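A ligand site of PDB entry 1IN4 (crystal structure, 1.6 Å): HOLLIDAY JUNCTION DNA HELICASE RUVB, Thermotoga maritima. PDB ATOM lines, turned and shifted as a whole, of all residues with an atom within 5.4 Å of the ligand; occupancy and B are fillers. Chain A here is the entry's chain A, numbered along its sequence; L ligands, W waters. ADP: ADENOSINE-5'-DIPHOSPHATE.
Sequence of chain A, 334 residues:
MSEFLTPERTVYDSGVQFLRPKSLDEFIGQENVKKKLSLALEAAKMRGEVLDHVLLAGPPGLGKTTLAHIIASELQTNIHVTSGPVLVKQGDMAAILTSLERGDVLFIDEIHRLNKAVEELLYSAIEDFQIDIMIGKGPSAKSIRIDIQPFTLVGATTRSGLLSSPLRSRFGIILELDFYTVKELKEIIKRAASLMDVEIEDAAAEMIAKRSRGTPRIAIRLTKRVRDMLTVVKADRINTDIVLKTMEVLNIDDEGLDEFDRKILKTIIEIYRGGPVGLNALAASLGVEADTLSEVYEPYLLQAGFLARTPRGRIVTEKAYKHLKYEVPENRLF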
ATOM      1  N   LEU A  19       3.048  22.914 -16.226  1.00  0.00           N
ATOM      2  CA  LEU A  19       3.744  23.249 -17.466  1.00  0.00           C
ATOM      3  C   LEU A  19       3.491  22.182 -18.533  1.00  0.00           C
ATOM      4  O   LEU A  19       3.875  22.338 -19.683  1.00  0.00           O
ATOM      5  CB  LEU A  19       5.251  23.374 -17.214  1.00  0.00           C
ATOM      6  CG  LEU A  19       5.703  24.547 -16.338  1.00  0.00           C
ATOM      7  CD1 LEU A  19       7.174  24.399 -16.014  1.00  0.00           C
ATOM      8  CD2 LEU A  19       5.446  25.862 -17.075  1.00  0.00           C
ATOM      9  N   ARG A  20       2.838  21.101 -18.120  1.00  0.00           N
ATOM     10  CA  ARG A  20       2.532  19.991 -19.025  1.00  0.00           C
ATOM     11  C   ARG A  20       1.286  20.238 -19.880  1.00  0.00           C
ATOM     12  O   ARG A  20       0.219  20.555 -19.347  1.00  0.00           O
ATOM     13  CB  ARG A  20       2.317  18.706 -18.230  1.00  0.00           C
ATOM     14  CG  ARG A  20       1.990  17.490 -19.083  1.00  0.00           C
ATOM     15  CD  ARG A  20       1.567  16.305 -18.215  1.00  0.00           C
ATOM     16  NE  ARG A  20       2.523  16.081 -17.129  1.00  0.00           N
ATOM     17  CZ  ARG A  20       3.812  15.815 -17.314  1.00  0.00           C
ATOM     18  NH1 ARG A  20       4.307  15.728 -18.544  1.00  0.00           N
ATOM     19  NH2 ARG A  20       4.606  15.635 -16.269  1.00  0.00           N
ATOM     20  N   PRO A  21       1.405  20.121 -21.209  1.00  0.00           N
ATOM     21  CA  PRO A  21       0.271  20.328 -22.112  1.00  0.00           C
ATOM     22  C   PRO A  21      -0.868  19.394 -21.709  1.00  0.00           C
ATOM     23  O   PRO A  21      -0.624  18.223 -21.424  1.00  0.00           O
ATOM     24  CB  PRO A  21       0.831  19.956 -23.479  1.00  0.00           C
ATOM     25  CG  PRO A  21       2.258  20.401 -23.361  1.00  0.00           C
ATOM     26  CD  PRO A  21       2.654  19.951 -21.971  1.00  0.00           C
ATOM     27  N   GLU A  26      -2.395  22.368 -26.961  1.00  0.00           N
ATOM     28  CA  GLU A  26      -1.400  22.989 -26.098  1.00  0.00           C
ATOM     29  C   GLU A  26      -0.029  22.367 -26.326  1.00  0.00           C
ATOM     30  O   GLU A  26       0.960  22.778 -25.718  1.00  0.00           O
ATOM     31  CB  GLU A  26      -1.766  22.820 -24.620  1.00  0.00           C
ATOM     32  CG  GLU A  26      -3.010  23.571 -24.206  1.00  0.00           C
ATOM     33  CD  GLU A  26      -3.364  23.363 -22.757  1.00  0.00           C
ATOM     34  OE1 GLU A  26      -4.451  23.838 -22.349  1.00  0.00           O
ATOM     35  OE2 GLU A  26      -2.574  22.753 -22.019  1.00  0.00           O
ATOM     36  N   PHE A  27       0.031  21.387 -27.222  1.00  0.00           N
ATOM     37  CA  PHE A  27       1.271  20.673 -27.525  1.00  0.00           C
ATOM     38  C   PHE A  27       1.974  21.311 -28.728  1.00  0.00           C
ATOM     39  O   PHE A  27       1.586  21.100 -29.877  1.00  0.00           O
ATOM     40  CB  PHE A  27       0.953  19.199 -27.790  1.00  0.00           C
ATOM     41  CG  PHE A  27       2.145  18.296 -27.737  1.00  0.00           C
ATOM     42  CD1 PHE A  27       2.936  18.071 -28.858  1.00  0.00           C
ATOM     43  CD2 PHE A  27       2.463  17.625 -26.548  1.00  0.00           C
ATOM     44  CE1 PHE A  27       4.015  17.196 -28.813  1.00  0.00           C
ATOM     45  CE2 PHE A  27       3.544  16.738 -26.491  1.00  0.00           C
ATOM     46  CZ  PHE A  27       4.324  16.528 -27.627  1.00  0.00           C
ATOM     47  N   ILE A  28       3.019  22.082 -28.454  1.00  0.00           N
ATOM     48  CA  ILE A  28       3.758  22.763 -29.505  1.00  0.00           C
ATOM     49  C   ILE A  28       4.683  21.819 -30.274  1.00  0.00           C
ATOM     50  O   ILE A  28       5.355  20.969 -29.688  1.00  0.00           O
ATOM     51  CB  ILE A  28       4.587  23.941 -28.906  1.00  0.00           C
ATOM     52  CG1 ILE A  28       3.632  25.067 -28.475  1.00  0.00           C
ATOM     53  CG2 ILE A  28       5.603  24.457 -29.925  1.00  0.00           C
ATOM     54  CD1 ILE A  28       4.296  26.156 -27.647  1.00  0.00           C
ATOM     55  N   GLY A  29       4.693  21.945 -31.599  1.00  0.00           N
ATOM     56  CA  GLY A  29       5.559  21.115 -32.412  1.00  0.00           C
ATOM     57  C   GLY A  29       5.024  19.730 -32.718  1.00  0.00           C
ATOM     58  O   GLY A  29       3.848  19.451 -32.470  1.00  0.00           O
ATOM     59  N   PRO A  59      13.756   9.838 -28.217  1.00  0.00           N
ATOM     60  CA  PRO A  59      14.560  10.154 -27.036  1.00  0.00           C
ATOM     61  C   PRO A  59      13.767  10.758 -25.879  1.00  0.00           C
ATOM     62  O   PRO A  59      12.658  11.279 -26.074  1.00  0.00           O
ATOM     63  CB  PRO A  59      15.622  11.108 -27.585  1.00  0.00           C
ATOM     64  CG  PRO A  59      14.945  11.746 -28.755  1.00  0.00           C
ATOM     65  CD  PRO A  59      14.218  10.582 -29.395  1.00  0.00           C
ATOM     66  N   PRO A  60      14.327  10.701 -24.661  1.00  0.00           N
ATOM     67  CA  PRO A  60      13.687  11.242 -23.458  1.00  0.00           C
ATOM     68  C   PRO A  60      13.404  12.730 -23.516  1.00  0.00           C
ATOM     69  O   PRO A  60      14.133  13.497 -24.160  1.00  0.00           O
ATOM     70  CB  PRO A  60      14.702  10.948 -22.348  1.00  0.00           C
ATOM     71  CG  PRO A  60      15.461   9.788 -22.871  1.00  0.00           C
ATOM     72  CD  PRO A  60      15.621  10.096 -24.329  1.00  0.00           C
ATOM     73  N   GLY A  61      12.345  13.121 -22.799  1.00  0.00           N
ATOM     74  CA  GLY A  61      11.958  14.515 -22.690  1.00  0.00           C
ATOM     75  C   GLY A  61      11.292  15.136 -23.899  1.00  0.00           C
ATOM     76  O   GLY A  61      11.141  16.354 -23.952  1.00  0.00           O
ATOM     77  N   LEU A  62      10.877  14.299 -24.855  1.00  0.00           N
ATOM     78  CA  LEU A  62      10.238  14.783 -26.091  1.00  0.00           C
ATOM     79  C   LEU A  62       8.727  14.850 -26.028  1.00  0.00           C
ATOM     80  O   LEU A  62       8.091  15.283 -27.001  1.00  0.00           O
ATOM     81  CB  LEU A  62      10.626  13.893 -27.272  1.00  0.00           C
ATOM     82  CG  LEU A  62      12.096  13.914 -27.714  1.00  0.00           C
ATOM     83  CD1 LEU A  62      12.222  13.182 -29.043  1.00  0.00           C
ATOM     84  CD2 LEU A  62      12.584  15.356 -27.847  1.00  0.00           C
ATOM     85  N   GLY A  63       8.139  14.416 -24.918  1.00  0.00           N
ATOM     86  CA  GLY A  63       6.699  14.455 -24.780  1.00  0.00           C
ATOM     87  C   GLY A  63       5.900  13.178 -24.906  1.00  0.00           C
ATOM     88  O   GLY A  63       4.676  13.240 -25.052  1.00  0.00           O
ATOM     89  N   LYS A  64       6.550  12.010 -24.863  1.00  0.00           N
ATOM     90  CA  LYS A  64       5.849  10.720 -24.988  1.00  0.00           C
ATOM     91  C   LYS A  64       4.835  10.528 -23.856  1.00  0.00           C
ATOM     92  O   LYS A  64       3.672  10.197 -24.101  1.00  0.00           O
ATOM     93  CB  LYS A  64       6.846   9.543 -25.015  1.00  0.00           C
ATOM     94  CG  LYS A  64       7.903   9.699 -26.118  1.00  0.00           C
ATOM     95  CD  LYS A  64       8.797   8.470 -26.328  1.00  0.00           C
ATOM     96  CE  LYS A  64       9.743   8.225 -25.160  1.00  0.00           C
ATOM     97  NZ  LYS A  64      10.642   9.393 -24.948  1.00  0.00           N
ATOM     98  N   THR A  65       5.286  10.734 -22.623  1.00  0.00           N
ATOM     99  CA  THR A  65       4.451  10.629 -21.448  1.00  0.00           C
ATOM    100  C   THR A  65       3.304  11.643 -21.552  1.00  0.00           C
ATOM    101  O   THR A  65       2.141  11.336 -21.277  1.00  0.00           O
ATOM    102  CB  THR A  65       5.265  10.910 -20.187  1.00  0.00           C
ATOM    103  OG1 THR A  65       6.217   9.845 -19.988  1.00  0.00           O
ATOM    104  CG2 THR A  65       4.354  11.085 -18.959  1.00  0.00           C
ATOM    105  N   THR A  66       3.639  12.860 -21.953  1.00  0.00           N
ATOM    106  CA  THR A  66       2.642  13.919 -22.107  1.00  0.00           C
ATOM    107  C   THR A  66       1.556  13.472 -23.081  1.00  0.00           C
ATOM    108  O   THR A  66       0.360  13.619 -22.803  1.00  0.00           O
ATOM    109  CB  THR A  66       3.323  15.203 -22.597  1.00  0.00           C
ATOM    110  OG1 THR A  66       4.297  15.606 -21.632  1.00  0.00           O
ATOM    111  CG2 THR A  66       2.322  16.332 -22.795  1.00  0.00           C
ATOM    112  N   LEU A  67       1.956  12.906 -24.222  1.00  0.00           N
ATOM    113  CA  LEU A  67       0.972  12.446 -25.205  1.00  0.00           C
ATOM    114  C   LEU A  67       0.098  11.317 -24.686  1.00  0.00           C
ATOM    115  O   LEU A  67      -1.076  11.262 -25.024  1.00  0.00           O
ATOM    116  CB  LEU A  67       1.682  12.006 -26.493  1.00  0.00           C
ATOM    117  CG  LEU A  67       2.292  13.166 -27.287  1.00  0.00           C
ATOM    118  CD1 LEU A  67       3.220  12.632 -28.368  1.00  0.00           C
ATOM    119  CD2 LEU A  67       1.170  14.020 -27.883  1.00  0.00           C
ATOM    120  N   ASP A 109       5.628   2.775 -19.850  1.00  0.00           N
ATOM    121  CA  ASP A 109       6.857   3.458 -20.244  1.00  0.00           C
ATOM    122  C   ASP A 109       7.973   2.419 -20.266  1.00  0.00           C
ATOM    123  O   ASP A 109       7.916   1.436 -19.517  1.00  0.00           O
ATOM    124  CB  ASP A 109       7.164   4.573 -19.239  1.00  0.00           C
ATOM    125  CG  ASP A 109       8.278   5.472 -19.710  1.00  0.00           C
ATOM    126  OD1 ASP A 109       8.345   5.765 -20.925  1.00  0.00           O
ATOM    127  OD2 ASP A 109       9.077   5.922 -18.857  1.00  0.00           O
ATOM    128  N   TYR A 180      12.966  18.581 -31.562  1.00  0.00           N
ATOM    129  CA  TYR A 180      12.232  19.783 -31.974  1.00  0.00           C
ATOM    130  C   TYR A 180      13.136  20.829 -32.614  1.00  0.00           C
ATOM    131  O   TYR A 180      14.355  20.832 -32.412  1.00  0.00           O
ATOM    132  CB  TYR A 180      11.530  20.424 -30.795  1.00  0.00           C
ATOM    133  CG  TYR A 180      10.438  19.601 -30.167  1.00  0.00           C
ATOM    134  CD1 TYR A 180      10.722  18.371 -29.557  1.00  0.00           C
ATOM    135  CD2 TYR A 180       9.127  20.055 -30.160  1.00  0.00           C
ATOM    136  CE1 TYR A 180       9.690  17.622 -28.963  1.00  0.00           C
ATOM    137  CE2 TYR A 180       8.116  19.332 -29.568  1.00  0.00           C
ATOM    138  CZ  TYR A 180       8.397  18.115 -28.969  1.00  0.00           C
ATOM    139  OH  TYR A 180       7.333  17.450 -28.399  1.00  0.00           O
ATOM    140  N   ILE A 188       8.088  27.041 -26.722  1.00  0.00           N
ATOM    141  CA  ILE A 188       7.858  26.294 -25.481  1.00  0.00           C
ATOM    142  C   ILE A 188       8.441  27.069 -24.306  1.00  0.00           C
ATOM    143  O   ILE A 188       7.849  27.130 -23.232  1.00  0.00           O
ATOM    144  CB  ILE A 188       8.503  24.878 -25.571  1.00  0.00           C
ATOM    145  CG1 ILE A 188       7.743  24.043 -26.621  1.00  0.00           C
ATOM    146  CG2 ILE A 188       8.456  24.144 -24.222  1.00  0.00           C
ATOM    147  CD1 ILE A 188       8.383  22.714 -26.942  1.00  0.00           C
ATOM    148  N   ARG A 191       6.347  30.097 -23.475  1.00  0.00           N
ATOM    149  CA  ARG A 191       5.144  29.606 -22.807  1.00  0.00           C
ATOM    150  C   ARG A 191       5.460  29.289 -21.350  1.00  0.00           C
ATOM    151  O   ARG A 191       4.688  29.607 -20.459  1.00  0.00           O
ATOM    152  CB  ARG A 191       4.642  28.335 -23.512  1.00  0.00           C
ATOM    153  CG  ARG A 191       3.503  27.597 -22.825  1.00  0.00           C
ATOM    154  CD  ARG A 191       3.123  26.351 -23.605  1.00  0.00           C
ATOM    155  NE  ARG A 191       1.964  25.657 -23.046  1.00  0.00           N
ATOM    156  CZ  ARG A 191       2.011  24.807 -22.034  1.00  0.00           C
ATOM    157  NH1 ARG A 191       0.897  24.235 -21.593  1.00  0.00           N
ATOM    158  NH2 ARG A 191       3.169  24.498 -21.454  1.00  0.00           N
ATOM    159  N   PRO A 216      12.270  19.504 -25.183  1.00  0.00           N
ATOM    160  CA  PRO A 216      11.455  20.386 -24.322  1.00  0.00           C
ATOM    161  C   PRO A 216      11.834  20.302 -22.848  1.00  0.00           C
ATOM    162  O   PRO A 216      11.943  21.326 -22.170  1.00  0.00           O
ATOM    163  CB  PRO A 216      10.029  19.889 -24.575  1.00  0.00           C
ATOM    164  CG  PRO A 216      10.091  19.472 -26.030  1.00  0.00           C
ATOM    165  CD  PRO A 216      11.418  18.747 -26.129  1.00  0.00           C
ATOM    166  N   ARG A 217      12.021  19.087 -22.315  1.00  0.00           N
ATOM    167  CA  ARG A 217      12.385  18.914 -20.918  1.00  0.00           C
ATOM    168  C   ARG A 217      13.634  19.741 -20.579  1.00  0.00           C
ATOM    169  O   ARG A 217      13.679  20.427 -19.559  1.00  0.00           O
ATOM    170  CB  ARG A 217      12.642  17.436 -20.618  1.00  0.00           C
ATOM    171  CG  ARG A 217      13.079  17.115 -19.181  1.00  0.00           C
ATOM    172  CD  ARG A 217      13.362  15.619 -19.002  1.00  0.00           C
ATOM    173  NE  ARG A 217      12.155  14.805 -18.945  1.00  0.00           N
ATOM    174  CZ  ARG A 217      12.138  13.474 -18.975  1.00  0.00           C
ATOM    175  NH1 ARG A 217      13.280  12.801 -19.058  1.00  0.00           N
ATOM    176  NH2 ARG A 217      10.989  12.813 -18.918  1.00  0.00           N
ATOM    177  N   ILE A 220      12.846  23.610 -20.685  1.00  0.00           N
ATOM    178  CA  ILE A 220      12.082  24.105 -19.541  1.00  0.00           C
ATOM    179  C   ILE A 220      12.947  24.190 -18.297  1.00  0.00           C
ATOM    180  O   ILE A 220      12.819  25.142 -17.522  1.00  0.00           O
ATOM    181  CB  ILE A 220      10.832  23.216 -19.264  1.00  0.00           C
ATOM    182  CG1 ILE A 220       9.860  23.314 -20.450  1.00  0.00           C
ATOM    183  CG2 ILE A 220      10.140  23.670 -17.955  1.00  0.00           C
ATOM    184  CD1 ILE A 220       9.025  22.055 -20.637  1.00  0.00           C
HETATM  185  PB  ADP L   1       9.061  11.771 -22.339  1.00  0.00           P
HETATM  186  O1B ADP L   1       9.207  11.720 -23.807  1.00  0.00           O
HETATM  187  O2B ADP L   1       7.973  10.822 -21.780  1.00  0.00           O
HETATM  188  O3B ADP L   1      10.376  11.542 -21.573  1.00  0.00           O
HETATM  189  PA  ADP L   1       7.555  13.992 -21.136  1.00  0.00           P
HETATM  190  O1A ADP L   1       6.201  13.770 -21.741  1.00  0.00           O
HETATM  191  O2A ADP L   1       7.649  13.539 -19.732  1.00  0.00           O
HETATM  192  O3A ADP L   1       8.736  13.236 -21.966  1.00  0.00           O
HETATM  193  O5' ADP L   1       7.972  15.499 -21.244  1.00  0.00           O
HETATM  194  C5' ADP L   1       8.946  16.360 -20.701  1.00  0.00           C
HETATM  195  C4' ADP L   1       8.614  17.610 -20.207  1.00  0.00           C
HETATM  196  O4' ADP L   1       8.593  18.381 -21.354  1.00  0.00           O
HETATM  197  C3' ADP L   1       7.128  17.766 -19.809  1.00  0.00           C
HETATM  198  O3' ADP L   1       7.335  18.617 -18.685  1.00  0.00           O
HETATM  199  C2' ADP L   1       6.364  18.551 -20.716  1.00  0.00           C
HETATM  200  O2' ADP L   1       5.274  19.169 -20.004  1.00  0.00           O
HETATM  201  C1' ADP L   1       7.477  18.957 -21.771  1.00  0.00           C
HETATM  202  N9  ADP L   1       7.049  18.830 -23.078  1.00  0.00           N
HETATM  203  C8  ADP L   1       7.170  17.791 -23.948  1.00  0.00           C
HETATM  204  N7  ADP L   1       6.695  18.001 -25.075  1.00  0.00           N
HETATM  205  C5  ADP L   1       6.208  19.269 -25.006  1.00  0.00           C
HETATM  206  C6  ADP L   1       5.544  20.144 -25.972  1.00  0.00           C
HETATM  207  N6  ADP L   1       5.300  19.708 -27.240  1.00  0.00           N
HETATM  208  N1  ADP L   1       5.146  21.445 -25.573  1.00  0.00           N
HETATM  209  C2  ADP L   1       5.406  21.881 -24.265  1.00  0.00           C
HETATM  210  N3  ADP L   1       6.039  21.119 -23.308  1.00  0.00           N
HETATM  211  C4  ADP L   1       6.411  19.829 -23.741  1.00  0.00           C
HETATM  212  O   HOH W   1       6.137  14.100 -17.719  1.00  0.00           O
HETATM  213  O   HOH W   2       8.496  11.271 -18.220  1.00  0.00           O
HETATM  214  O   HOH W   3       5.994  22.923 -21.157  1.00  0.00           O
HETATM  215  O   HOH W   4       5.497  19.120 -16.670  1.00  0.00           O
HETATM  216  O   HOH W   5      11.706   8.471 -22.506  1.00  0.00           O
HETATM  217  O   HOH W   6       9.018   8.297 -21.687  1.00  0.00           O
HETATM  218  O   HOH W   7       3.474  23.499 -26.032  1.00  0.00           O
HETATM  219  O   HOH W   8       9.805  19.088 -17.077  1.00  0.00           O
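The backbone NH (N) of Lys 64 lies within hydrogen-bond range of an oxygen (O1B) of the ligand (2.9 Å). The backbone carbonyl oxygen of Leu 19 sits at hydrogen-bond distance from an oxygen (O2') of the ligand, 3.5 Å away. N of Thr 65 is in hydrogen-bond range of O2B of the ligand (2.8 Å). The backbone NH (N) of Gly 63 lies within hydrogen-bond range of an oxygen (O1B) of the ligand. O of Ile 28 is in hydrogen-bond range of N6 of the ligand (2.8 Å). OG1 of Thr 65 is in hydrogen-bond range of O2B of the ligand, 2.7 Å away. The guanidinium group of Arg 217 is in salt-bridge range of an oxygen (O3B) of the ligand (3.0 Å). The backbone NH of Leu 62 lies within hydrogen-bond range of an oxygen (O1B) of the ligand (3.2 Å). The side-chain hydroxyl (OH) of Tyr 180 lies within hydrogen-bond range of a nitrogen (N6) of the ligand, 3.3 Å away. The backbone NH (N) of Gly 61 lies within hydrogen-bond range of an oxygen (O3B) of the ligand (2.8 Å). The backbone NH of Thr 66 lies within hydrogen-bond range of an oxygen (O1A) of the ligand. The side-chain hydroxyl of Thr 66 lies within hydrogen-bond range of an oxygen (O1A) of the ligand (2.6 Å). O1B of the ligand is in salt-bridge range of NZ of Lys 64, 3.0 Å away.
The backbone carbonyl oxygen (O) of Leu 62 is in hydrogen-bond range of the side-chain hydroxyl (OH) of Tyr 180 (2.7 Å). The guanidinium group (NH1) of Arg 20 is in hydrogen-bond range of the side-chain hydroxyl (OG1) of Thr 66, 3.1 Å away. The backbone NH (N) of Arg 217 lies within hydrogen-bond range of the backbone carbonyl oxygen (O) of Gly 61. The backbone carbonyl oxygen (O) of Pro 59 sits at hydrogen-bond distance from the side-chain amino group (NZ) of Lys 64. The guanidinium group (NH2) of Arg 191 is in hydrogen-bond range of the backbone carbonyl oxygen (O) of Leu 19.
Merely in contact with the ligand: Arg 20 (3.0 Å), Pro 21 (3.4 Å), Phe 27 (3.2 Å), Pro 60 (3.8 Å), Ile 188 (3.7 Å), Pro 216 (3.5 Å) and Ile 220 (3.6 Å). Hydrophobic or aromatic side chains that line the ligand: Pro 21, Phe 27, Tyr 180, Ile 188, Pro 216 and Ile 220. Within 4 Å of the ligand: Leu 19, Arg 20, Pro 21, Phe 27, Ile 28, Pro 60, Gly 61, Leu 62, Gly 63, Lys 64, Thr 65, Thr 66, Tyr 180, Ile 188, Pro 216, Arg 217 and Ile 220. Along chain A the residues within 4 Å of the ligand span positions 19 to 220.
Water W1 lies within hydrogen-bond range of an oxygen (O2A) of the ligand (2.6 Å) and the guanidinium group (NH1) of Arg 20 (2.6 Å). Water W7 lies within hydrogen-bond range of the backbone carbonyl oxygen of Glu 26 (2.6 Å), a nitrogen (N1) of the ligand (2.7 Å) and the backbone NH of Ile 28 (2.8 Å). Water W6 lies within hydrogen-bond range of the side-chain carboxylate (OD1) of Asp 109 (2.7 Å) and an oxygen (O2B) of the ligand (2.7 Å). Water W3 lies within hydrogen-bond range of the backbone carbonyl oxygen of Leu 19 (2.6 Å), a nitrogen (N3) of the ligand (2.8 Å) and the guanidinium group of Arg 191 (3.2 Å). Water W2 lies within hydrogen-bond range of O2A of the ligand (2.9 Å), NH2 of Arg 217 (3.0 Å) and OG1 of Thr 65 (3.2 Å). Water W5 bridges NZ of Lys 64 and O3B of the ligand.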
